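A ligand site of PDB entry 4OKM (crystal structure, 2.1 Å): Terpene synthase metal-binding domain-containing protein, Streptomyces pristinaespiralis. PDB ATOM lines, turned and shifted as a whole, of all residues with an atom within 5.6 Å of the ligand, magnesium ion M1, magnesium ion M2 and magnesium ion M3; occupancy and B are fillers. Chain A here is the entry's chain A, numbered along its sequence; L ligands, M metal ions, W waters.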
ATOM      1  N   PHE A  79      -2.943  -5.785 -18.786  1.00  0.00           N
ATOM      2  CA  PHE A  79      -1.560  -6.266 -18.925  1.00  0.00           C
ATOM      3  C   PHE A  79      -0.874  -6.310 -17.550  1.00  0.00           C
ATOM      4  O   PHE A  79      -0.061  -7.186 -17.290  1.00  0.00           O
ATOM      5  CB  PHE A  79      -0.763  -5.419 -19.917  1.00  0.00           C
ATOM      6  CG  PHE A  79      -1.118  -5.672 -21.356  1.00  0.00           C
ATOM      7  CD1 PHE A  79      -1.509  -4.642 -22.189  1.00  0.00           C
ATOM      8  CD2 PHE A  79      -1.065  -6.963 -21.882  1.00  0.00           C
ATOM      9  CE1 PHE A  79      -1.835  -4.885 -23.511  1.00  0.00           C
ATOM     10  CE2 PHE A  79      -1.385  -7.213 -23.201  1.00  0.00           C
ATOM     11  CZ  PHE A  79      -1.780  -6.174 -24.013  1.00  0.00           C
ATOM     12  N   ASP A  82      -2.172  -9.622 -16.528  1.00  0.00           N
ATOM     13  CA  ASP A  82      -1.792 -10.702 -17.451  1.00  0.00           C
ATOM     14  C   ASP A  82      -0.263 -10.903 -17.538  1.00  0.00           C
ATOM     15  O   ASP A  82       0.218 -12.046 -17.503  1.00  0.00           O
ATOM     16  CB  ASP A  82      -2.387 -10.467 -18.846  1.00  0.00           C
ATOM     17  CG  ASP A  82      -2.589 -11.770 -19.613  1.00  0.00           C
ATOM     18  OD1 ASP A  82      -3.412 -12.596 -19.182  1.00  0.00           O
ATOM     19  OD2 ASP A  82      -1.918 -11.965 -20.646  1.00  0.00           O
ATOM     20  N   ASP A  83       0.486  -9.821 -17.659  1.00  0.00           N
ATOM     21  CA  ASP A  83       1.951  -9.893 -17.612  1.00  0.00           C
ATOM     22  C   ASP A  83       2.428 -10.083 -16.172  1.00  0.00           C
ATOM     23  O   ASP A  83       3.151 -11.034 -15.868  1.00  0.00           O
ATOM     24  CB  ASP A  83       2.598  -8.639 -18.204  1.00  0.00           C
ATOM     25  CG  ASP A  83       2.388  -8.508 -19.701  1.00  0.00           C
ATOM     26  OD1 ASP A  83       2.660  -7.419 -20.248  1.00  0.00           O
ATOM     27  OD2 ASP A  83       1.958  -9.493 -20.342  1.00  0.00           O
ATOM     28  N   GLU A  87       1.650 -14.393 -16.831  1.00  0.00           N
ATOM     29  CA  GLU A  87       2.725 -14.861 -17.730  1.00  0.00           C
ATOM     30  C   GLU A  87       4.163 -14.594 -17.256  1.00  0.00           C
ATOM     31  O   GLU A  87       5.087 -15.282 -17.702  1.00  0.00           O
ATOM     32  CB  GLU A  87       2.540 -14.273 -19.121  1.00  0.00           C
ATOM     33  CG  GLU A  87       1.197 -14.625 -19.747  1.00  0.00           C
ATOM     34  CD  GLU A  87       1.161 -14.382 -21.248  1.00  0.00           C
ATOM     35  OE1 GLU A  87       1.900 -15.057 -21.987  1.00  0.00           O
ATOM     36  OE2 GLU A  87       0.385 -13.502 -21.691  1.00  0.00           O
ATOM     37  N   VAL A 156      -7.728 -17.668 -17.629  1.00  0.00           N
ATOM     38  CA  VAL A 156      -6.290 -17.608 -17.328  1.00  0.00           C
ATOM     39  C   VAL A 156      -5.884 -18.522 -16.161  1.00  0.00           C
ATOM     40  O   VAL A 156      -4.711 -18.872 -16.037  1.00  0.00           O
ATOM     41  CB  VAL A 156      -5.730 -16.170 -17.127  1.00  0.00           C
ATOM     42  CG1 VAL A 156      -5.733 -15.424 -18.455  1.00  0.00           C
ATOM     43  CG2 VAL A 156      -6.444 -15.404 -16.036  1.00  0.00           C
ATOM     44  N   GLU A 159      -5.361 -21.527 -18.232  1.00  0.00           N
ATOM     45  CA  GLU A 159      -4.058 -21.365 -18.873  1.00  0.00           C
ATOM     46  C   GLU A 159      -2.911 -21.624 -17.885  1.00  0.00           C
ATOM     47  O   GLU A 159      -1.898 -22.235 -18.232  1.00  0.00           O
ATOM     48  CB  GLU A 159      -3.907 -19.964 -19.473  1.00  0.00           C
ATOM     49  CG  GLU A 159      -2.666 -19.782 -20.325  1.00  0.00           C
ATOM     50  CD  GLU A 159      -2.323 -18.309 -20.597  1.00  0.00           C
ATOM     51  OE1 GLU A 159      -2.204 -17.517 -19.643  1.00  0.00           O
ATOM     52  OE2 GLU A 159      -2.141 -17.959 -21.768  1.00  0.00           O
ATOM     53  N   ARG A 178      -8.882 -19.587 -25.562  1.00  0.00           N
ATOM     54  CA  ARG A 178      -8.387 -18.377 -26.210  1.00  0.00           C
ATOM     55  C   ARG A 178      -9.502 -17.384 -26.530  1.00  0.00           C
ATOM     56  O   ARG A 178      -9.272 -16.191 -26.638  1.00  0.00           O
ATOM     57  CB  ARG A 178      -7.610 -18.745 -27.483  1.00  0.00           C
ATOM     58  CG  ARG A 178      -6.767 -17.635 -28.084  1.00  0.00           C
ATOM     59  CD  ARG A 178      -5.802 -17.025 -27.089  1.00  0.00           C
ATOM     60  NE  ARG A 178      -4.818 -16.158 -27.738  1.00  0.00           N
ATOM     61  CZ  ARG A 178      -4.254 -15.093 -27.169  1.00  0.00           C
ATOM     62  NH1 ARG A 178      -3.386 -14.362 -27.863  1.00  0.00           N
ATOM     63  NH2 ARG A 178      -4.552 -14.732 -25.918  1.00  0.00           N
ATOM     64  N   ASP A 181      -9.174 -15.766 -22.767  1.00  0.00           N
ATOM     65  CA  ASP A 181      -7.928 -15.470 -22.032  1.00  0.00           C
ATOM     66  C   ASP A 181      -7.100 -14.338 -22.622  1.00  0.00           C
ATOM     67  O   ASP A 181      -6.121 -13.921 -22.010  1.00  0.00           O
ATOM     68  CB  ASP A 181      -7.078 -16.750 -21.781  1.00  0.00           C
ATOM     69  CG  ASP A 181      -6.240 -17.181 -22.979  1.00  0.00           C
ATOM     70  OD1 ASP A 181      -5.678 -18.297 -22.894  1.00  0.00           O
ATOM     71  OD2 ASP A 181      -6.111 -16.456 -23.982  1.00  0.00           O
ATOM     72  N   GLY A 182      -7.504 -13.848 -23.786  1.00  0.00           N
ATOM     73  CA  GLY A 182      -6.920 -12.643 -24.373  1.00  0.00           C
ATOM     74  C   GLY A 182      -7.592 -11.370 -23.889  1.00  0.00           C
ATOM     75  O   GLY A 182      -7.219 -10.272 -24.324  1.00  0.00           O
ATOM     76  N   ASN A 224      -3.106 -11.807 -33.004  1.00  0.00           N
ATOM     77  CA  ASN A 224      -2.116 -11.628 -31.953  1.00  0.00           C
ATOM     78  C   ASN A 224      -1.147 -12.809 -31.864  1.00  0.00           C
ATOM     79  O   ASN A 224       0.062 -12.604 -31.768  1.00  0.00           O
ATOM     80  CB  ASN A 224      -2.769 -11.390 -30.592  1.00  0.00           C
ATOM     81  CG  ASN A 224      -1.752 -11.349 -29.474  1.00  0.00           C
ATOM     82  OD1 ASN A 224      -1.363 -12.394 -28.944  1.00  0.00           O
ATOM     83  ND2 ASN A 224      -1.305 -10.160 -29.108  1.00  0.00           N
ATOM     84  N   ASP A 225      -1.666 -14.027 -31.899  1.00  0.00           N
ATOM     85  CA  ASP A 225      -0.797 -15.211 -31.915  1.00  0.00           C
ATOM     86  C   ASP A 225       0.236 -15.110 -33.043  1.00  0.00           C
ATOM     87  O   ASP A 225       1.405 -15.459 -32.841  1.00  0.00           O
ATOM     88  CB  ASP A 225      -1.597 -16.507 -32.053  1.00  0.00           C
ATOM     89  CG  ASP A 225      -2.327 -16.884 -30.776  1.00  0.00           C
ATOM     90  OD1 ASP A 225      -2.950 -17.970 -30.761  1.00  0.00           O
ATOM     91  OD2 ASP A 225      -2.279 -16.113 -29.787  1.00  0.00           O
ATOM     92  N   SER A 228       2.524 -11.669 -32.251  1.00  0.00           N
ATOM     93  CA  SER A 228       3.278 -11.771 -30.991  1.00  0.00           C
ATOM     94  C   SER A 228       4.096 -13.062 -30.880  1.00  0.00           C
ATOM     95  O   SER A 228       4.809 -13.250 -29.894  1.00  0.00           O
ATOM     96  CB  SER A 228       2.338 -11.631 -29.780  1.00  0.00           C
ATOM     97  OG  SER A 228       1.553 -12.793 -29.532  1.00  0.00           O
ATOM     98  N   LYS A 231       7.849 -12.257 -30.332  1.00  0.00           N
ATOM     99  CA  LYS A 231       8.038 -11.778 -28.957  1.00  0.00           C
ATOM    100  C   LYS A 231       7.901 -12.916 -27.919  1.00  0.00           C
ATOM    101  O   LYS A 231       8.623 -12.950 -26.928  1.00  0.00           O
ATOM    102  CB  LYS A 231       7.023 -10.642 -28.682  1.00  0.00           C
ATOM    103  CG  LYS A 231       6.871 -10.228 -27.235  1.00  0.00           C
ATOM    104  CD  LYS A 231       5.861 -11.098 -26.485  1.00  0.00           C
ATOM    105  CE  LYS A 231       4.499 -10.448 -26.332  1.00  0.00           C
ATOM    106  NZ  LYS A 231       3.815 -11.005 -25.130  1.00  0.00           N
ATOM    107  N   GLU A 232       6.984 -13.846 -28.167  1.00  0.00           N
ATOM    108  CA  GLU A 232       6.708 -14.935 -27.239  1.00  0.00           C
ATOM    109  C   GLU A 232       7.715 -16.078 -27.348  1.00  0.00           C
ATOM    110  O   GLU A 232       8.261 -16.526 -26.332  1.00  0.00           O
ATOM    111  CB  GLU A 232       5.281 -15.465 -27.436  1.00  0.00           C
ATOM    112  CG  GLU A 232       4.234 -14.505 -26.891  1.00  0.00           C
ATOM    113  CD  GLU A 232       2.815 -14.845 -27.325  1.00  0.00           C
ATOM    114  OE1 GLU A 232       1.911 -14.021 -27.033  1.00  0.00           O
ATOM    115  OE2 GLU A 232       2.600 -15.906 -27.957  1.00  0.00           O
ATOM    116  N   LEU A 240       2.100 -19.887 -24.909  1.00  0.00           N
ATOM    117  CA  LEU A 240       1.081 -20.611 -25.667  1.00  0.00           C
ATOM    118  C   LEU A 240       0.593 -19.739 -26.793  1.00  0.00           C
ATOM    119  O   LEU A 240       0.386 -18.536 -26.604  1.00  0.00           O
ATOM    120  CB  LEU A 240      -0.119 -20.956 -24.785  1.00  0.00           C
ATOM    121  CG  LEU A 240      -0.428 -22.411 -24.483  1.00  0.00           C
ATOM    122  CD1 LEU A 240      -1.768 -22.497 -23.763  1.00  0.00           C
ATOM    123  CD2 LEU A 240      -0.434 -23.253 -25.740  1.00  0.00           C
ATOM    124  N   TRP A 304      -2.271  -1.957 -34.489  1.00  0.00           N
ATOM    125  CA  TRP A 304      -1.465  -1.877 -33.259  1.00  0.00           C
ATOM    126  C   TRP A 304      -0.512  -3.070 -33.144  1.00  0.00           C
ATOM    127  O   TRP A 304       0.617  -2.926 -32.690  1.00  0.00           O
ATOM    128  CB  TRP A 304      -2.386  -1.807 -32.048  1.00  0.00           C
ATOM    129  CG  TRP A 304      -1.699  -1.665 -30.720  1.00  0.00           C
ATOM    130  CD1 TRP A 304      -0.998  -0.585 -30.264  1.00  0.00           C
ATOM    131  CD2 TRP A 304      -1.684  -2.635 -29.660  1.00  0.00           C
ATOM    132  NE1 TRP A 304      -0.535  -0.828 -28.987  1.00  0.00           N
ATOM    133  CE2 TRP A 304      -0.946  -2.070 -28.597  1.00  0.00           C
ATOM    134  CE3 TRP A 304      -2.225  -3.914 -29.508  1.00  0.00           C
ATOM    135  CZ2 TRP A 304      -0.728  -2.749 -27.403  1.00  0.00           C
ATOM    136  CZ3 TRP A 304      -2.010  -4.581 -28.311  1.00  0.00           C
ATOM    137  CH2 TRP A 304      -1.270  -4.000 -27.274  1.00  0.00           C
ATOM    138  N   ARG A 310       5.685  -3.522 -28.165  1.00  0.00           N
ATOM    139  CA  ARG A 310       5.327  -4.771 -27.506  1.00  0.00           C
ATOM    140  C   ARG A 310       5.539  -5.966 -28.439  1.00  0.00           C
ATOM    141  O   ARG A 310       5.913  -7.051 -28.004  1.00  0.00           O
ATOM    142  CB  ARG A 310       3.868  -4.737 -27.038  1.00  0.00           C
ATOM    143  CG  ARG A 310       3.457  -5.939 -26.207  1.00  0.00           C
ATOM    144  CD  ARG A 310       2.020  -5.850 -25.724  1.00  0.00           C
ATOM    145  NE  ARG A 310       1.714  -7.033 -24.934  1.00  0.00           N
ATOM    146  CZ  ARG A 310       1.958  -7.196 -23.629  1.00  0.00           C
ATOM    147  NH1 ARG A 310       1.644  -8.343 -23.051  1.00  0.00           N
ATOM    148  NH2 ARG A 310       2.512  -6.227 -22.901  1.00  0.00           N
ATOM    149  N   TYR A 311       5.300  -5.757 -29.744  1.00  0.00           N
ATOM    150  CA  TYR A 311       5.428  -6.840 -30.733  1.00  0.00           C
ATOM    151  C   TYR A 311       6.619  -6.661 -31.688  1.00  0.00           C
ATOM    152  O   TYR A 311       7.202  -7.658 -32.139  1.00  0.00           O
ATOM    153  CB  TYR A 311       4.107  -6.989 -31.503  1.00  0.00           C
ATOM    154  CG  TYR A 311       2.906  -7.086 -30.586  1.00  0.00           C
ATOM    155  CD1 TYR A 311       1.923  -6.090 -30.586  1.00  0.00           C
ATOM    156  CD2 TYR A 311       2.780  -8.125 -29.683  1.00  0.00           C
ATOM    157  CE1 TYR A 311       0.840  -6.168 -29.727  1.00  0.00           C
ATOM    158  CE2 TYR A 311       1.695  -8.213 -28.815  1.00  0.00           C
ATOM    159  CZ  TYR A 311       0.730  -7.229 -28.836  1.00  0.00           C
ATOM    160  OH  TYR A 311      -0.336  -7.294 -27.979  1.00  0.00           O
HETATM  161  O1  LIG L   1       0.105  -8.937 -26.017  1.00  0.00           O
HETATM  162  P1  LIG L   1       0.261 -10.419 -25.796  1.00  0.00           P
HETATM  163  O2  LIG L   1       0.648 -11.212 -27.033  1.00  0.00           O
HETATM  164  O3  LIG L   1       1.077 -10.755 -24.584  1.00  0.00           O
HETATM  165  O4  LIG L   1      -1.244 -10.892 -25.443  1.00  0.00           O
HETATM  166  P2  LIG L   1      -1.613 -12.427 -25.074  1.00  0.00           P
HETATM  167  O5  LIG L   1      -3.118 -12.409 -25.040  1.00  0.00           O
HETATM  168  O6  LIG L   1      -0.962 -12.662 -23.732  1.00  0.00           O
HETATM  169  O7  LIG L   1      -1.037 -13.273 -26.183  1.00  0.00           O
HETATM  170 MG    MG M   1       0.868 -11.970 -23.085  1.00  0.00          MG
HETATM  171 MG    MG M   2      -1.744 -13.696 -21.868  1.00  0.00          MG
HETATM  172 MG    MG M   3       0.217 -13.095 -27.692  1.00  0.00          MG
HETATM  173  O   HOH W   1       1.928 -13.420 -24.192  1.00  0.00           O
HETATM  174  O   HOH W   2      -3.572 -13.298 -22.536  1.00  0.00           O
HETATM  175  O   HOH W   3       2.682 -11.438 -22.092  1.00  0.00           O
HETATM  176  O   HOH W   4      -0.316 -15.785 -25.318  1.00  0.00           O
HETATM  177  O   HOH W   5      -2.076 -14.834 -20.124  1.00  0.00           O
HETATM  178  O   HOH W   6      -0.143 -15.064 -28.587  1.00  0.00           O
HETATM  179  O   HOH W   7      -1.417 -15.492 -22.866  1.00  0.00           O
HETATM  180  O   HOH W   8      -0.090 -10.504 -21.924  1.00  0.00           O
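The side-chain hydroxyl (OH) of Tyr 311 is in hydrogen-bond range of an oxygen (O1) of the ligand (2.6 Å).
NE of Arg 310 is in salt-bridge range of O1 of the ligand (2.7 Å).
An oxygen (O3) of the ligand lies close to the side-chain amino group (NZ) of Lys 231 (2.8 Å).
O5 of the ligand is in salt-bridge range of NH2 of Arg 178 (2.9 Å).
ND2 of Asn 224 lies within hydrogen-bond range of OH of Tyr 311, 3.2 Å away.
OD1 of Asn 224 sits close to NH1 of Arg 178 (3.0 Å).
The guanidinium group (NH2) of Arg 310 lies within salt-bridge range of the side-chain carboxylate (OD1) of Asp 83 (2.9 Å).
The side-chain carboxylate (OD2) of Asp 181 lies within salt-bridge range of the guanidinium group (NH2) of Arg 178 (3.0 Å).
The side-chain carboxylate of Asp 225 is in salt-bridge range of the guanidinium group of Arg 178 (2.8 Å).
Merely in contact with the ligand: Phe 79 (3.6 Å) and Gly 182 (3.9 Å).
Hydrophobic or aromatic side chains within 4 Å of the ligand: Phe 79 and Tyr 311.
The nearest printed residue that does not touch the ligand is Asp 83 (4.5 Å).
Asp 83 touches magnesium ion M1.
Lys 231 touches magnesium ion M1.
Arg 310 touches magnesium ion M1 (NH1 to MG, 3.7 Å).
Five residues have an atom within 4 Å of magnesium ion M1: Asp 82, Asp 83, Glu 87, Lys 231 and Arg 310.
The nearest printed residue that does not touch magnesium ion M2 is Glu 159 (4.3 Å).
Residues that only touch magnesium ion M3: Arg 178 (3.8 Å).
Within 4 Å of magnesium ion M3: Arg 178, Asn 224, Ser 228 and Glu 232.
The nearest printed residue that does not touch magnesium ion M3 is Asp 225 (4.4 Å).
Magnesium ion M1 is bound by an oxygen (O3) of the ligand (1.9 Å), an oxygen (O6) of the ligand (2.1 Å), water W8 (2.1 Å), water W1 (2.1 Å), the side-chain carboxylate (OE2) of Glu 87 (2.1 Å) and water W3 (2.1 Å).
Magnesium ion M2 is bound by water W2 (2.0 Å), water W7 (2.1 Å), water W5 (2.1 Å), the side-chain carboxylate of Asp 82 (2.1 Å), the side-chain carboxylate of Glu 87 (2.1 Å) and an oxygen (O6) of the ligand (2.3 Å).
Magnesium ion M2 has six donor atoms within binding distance.
Magnesium ion M3 is bound by O7 of the ligand (2.0 Å), OE1 of Glu 232 (2.0 Å), O2 of the ligand (2.0 Å), OD1 of Asn 224 (2.1 Å), water W6 (2.2 Å) and OG of Ser 228 (2.3 Å).
Water W8 lies within hydrogen-bond range of the side-chain carboxylate (OD2) of Asp 83 (2.8 Å) and the guanidinium group (NH1) of Arg 310 (3.0 Å).
Water W1 bridges OE1 of Glu 87 and NZ of Lys 231.
Water W5 lies within hydrogen-bond range of OE1 of Glu 159 (2.7 Å) and OD1 of Asp 82 (2.8 Å).
Water W7 bridges OE2 of Glu 159 and OE1 of Glu 87.
Water W2 lies within hydrogen-bond range of O of Asp 181, O5 of the ligand and OD1 of Asp 82.
Water W6 lies within hydrogen-bond range of OD2 of Asp 225, OE2 of Glu 232 and NH1 of Arg 178.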
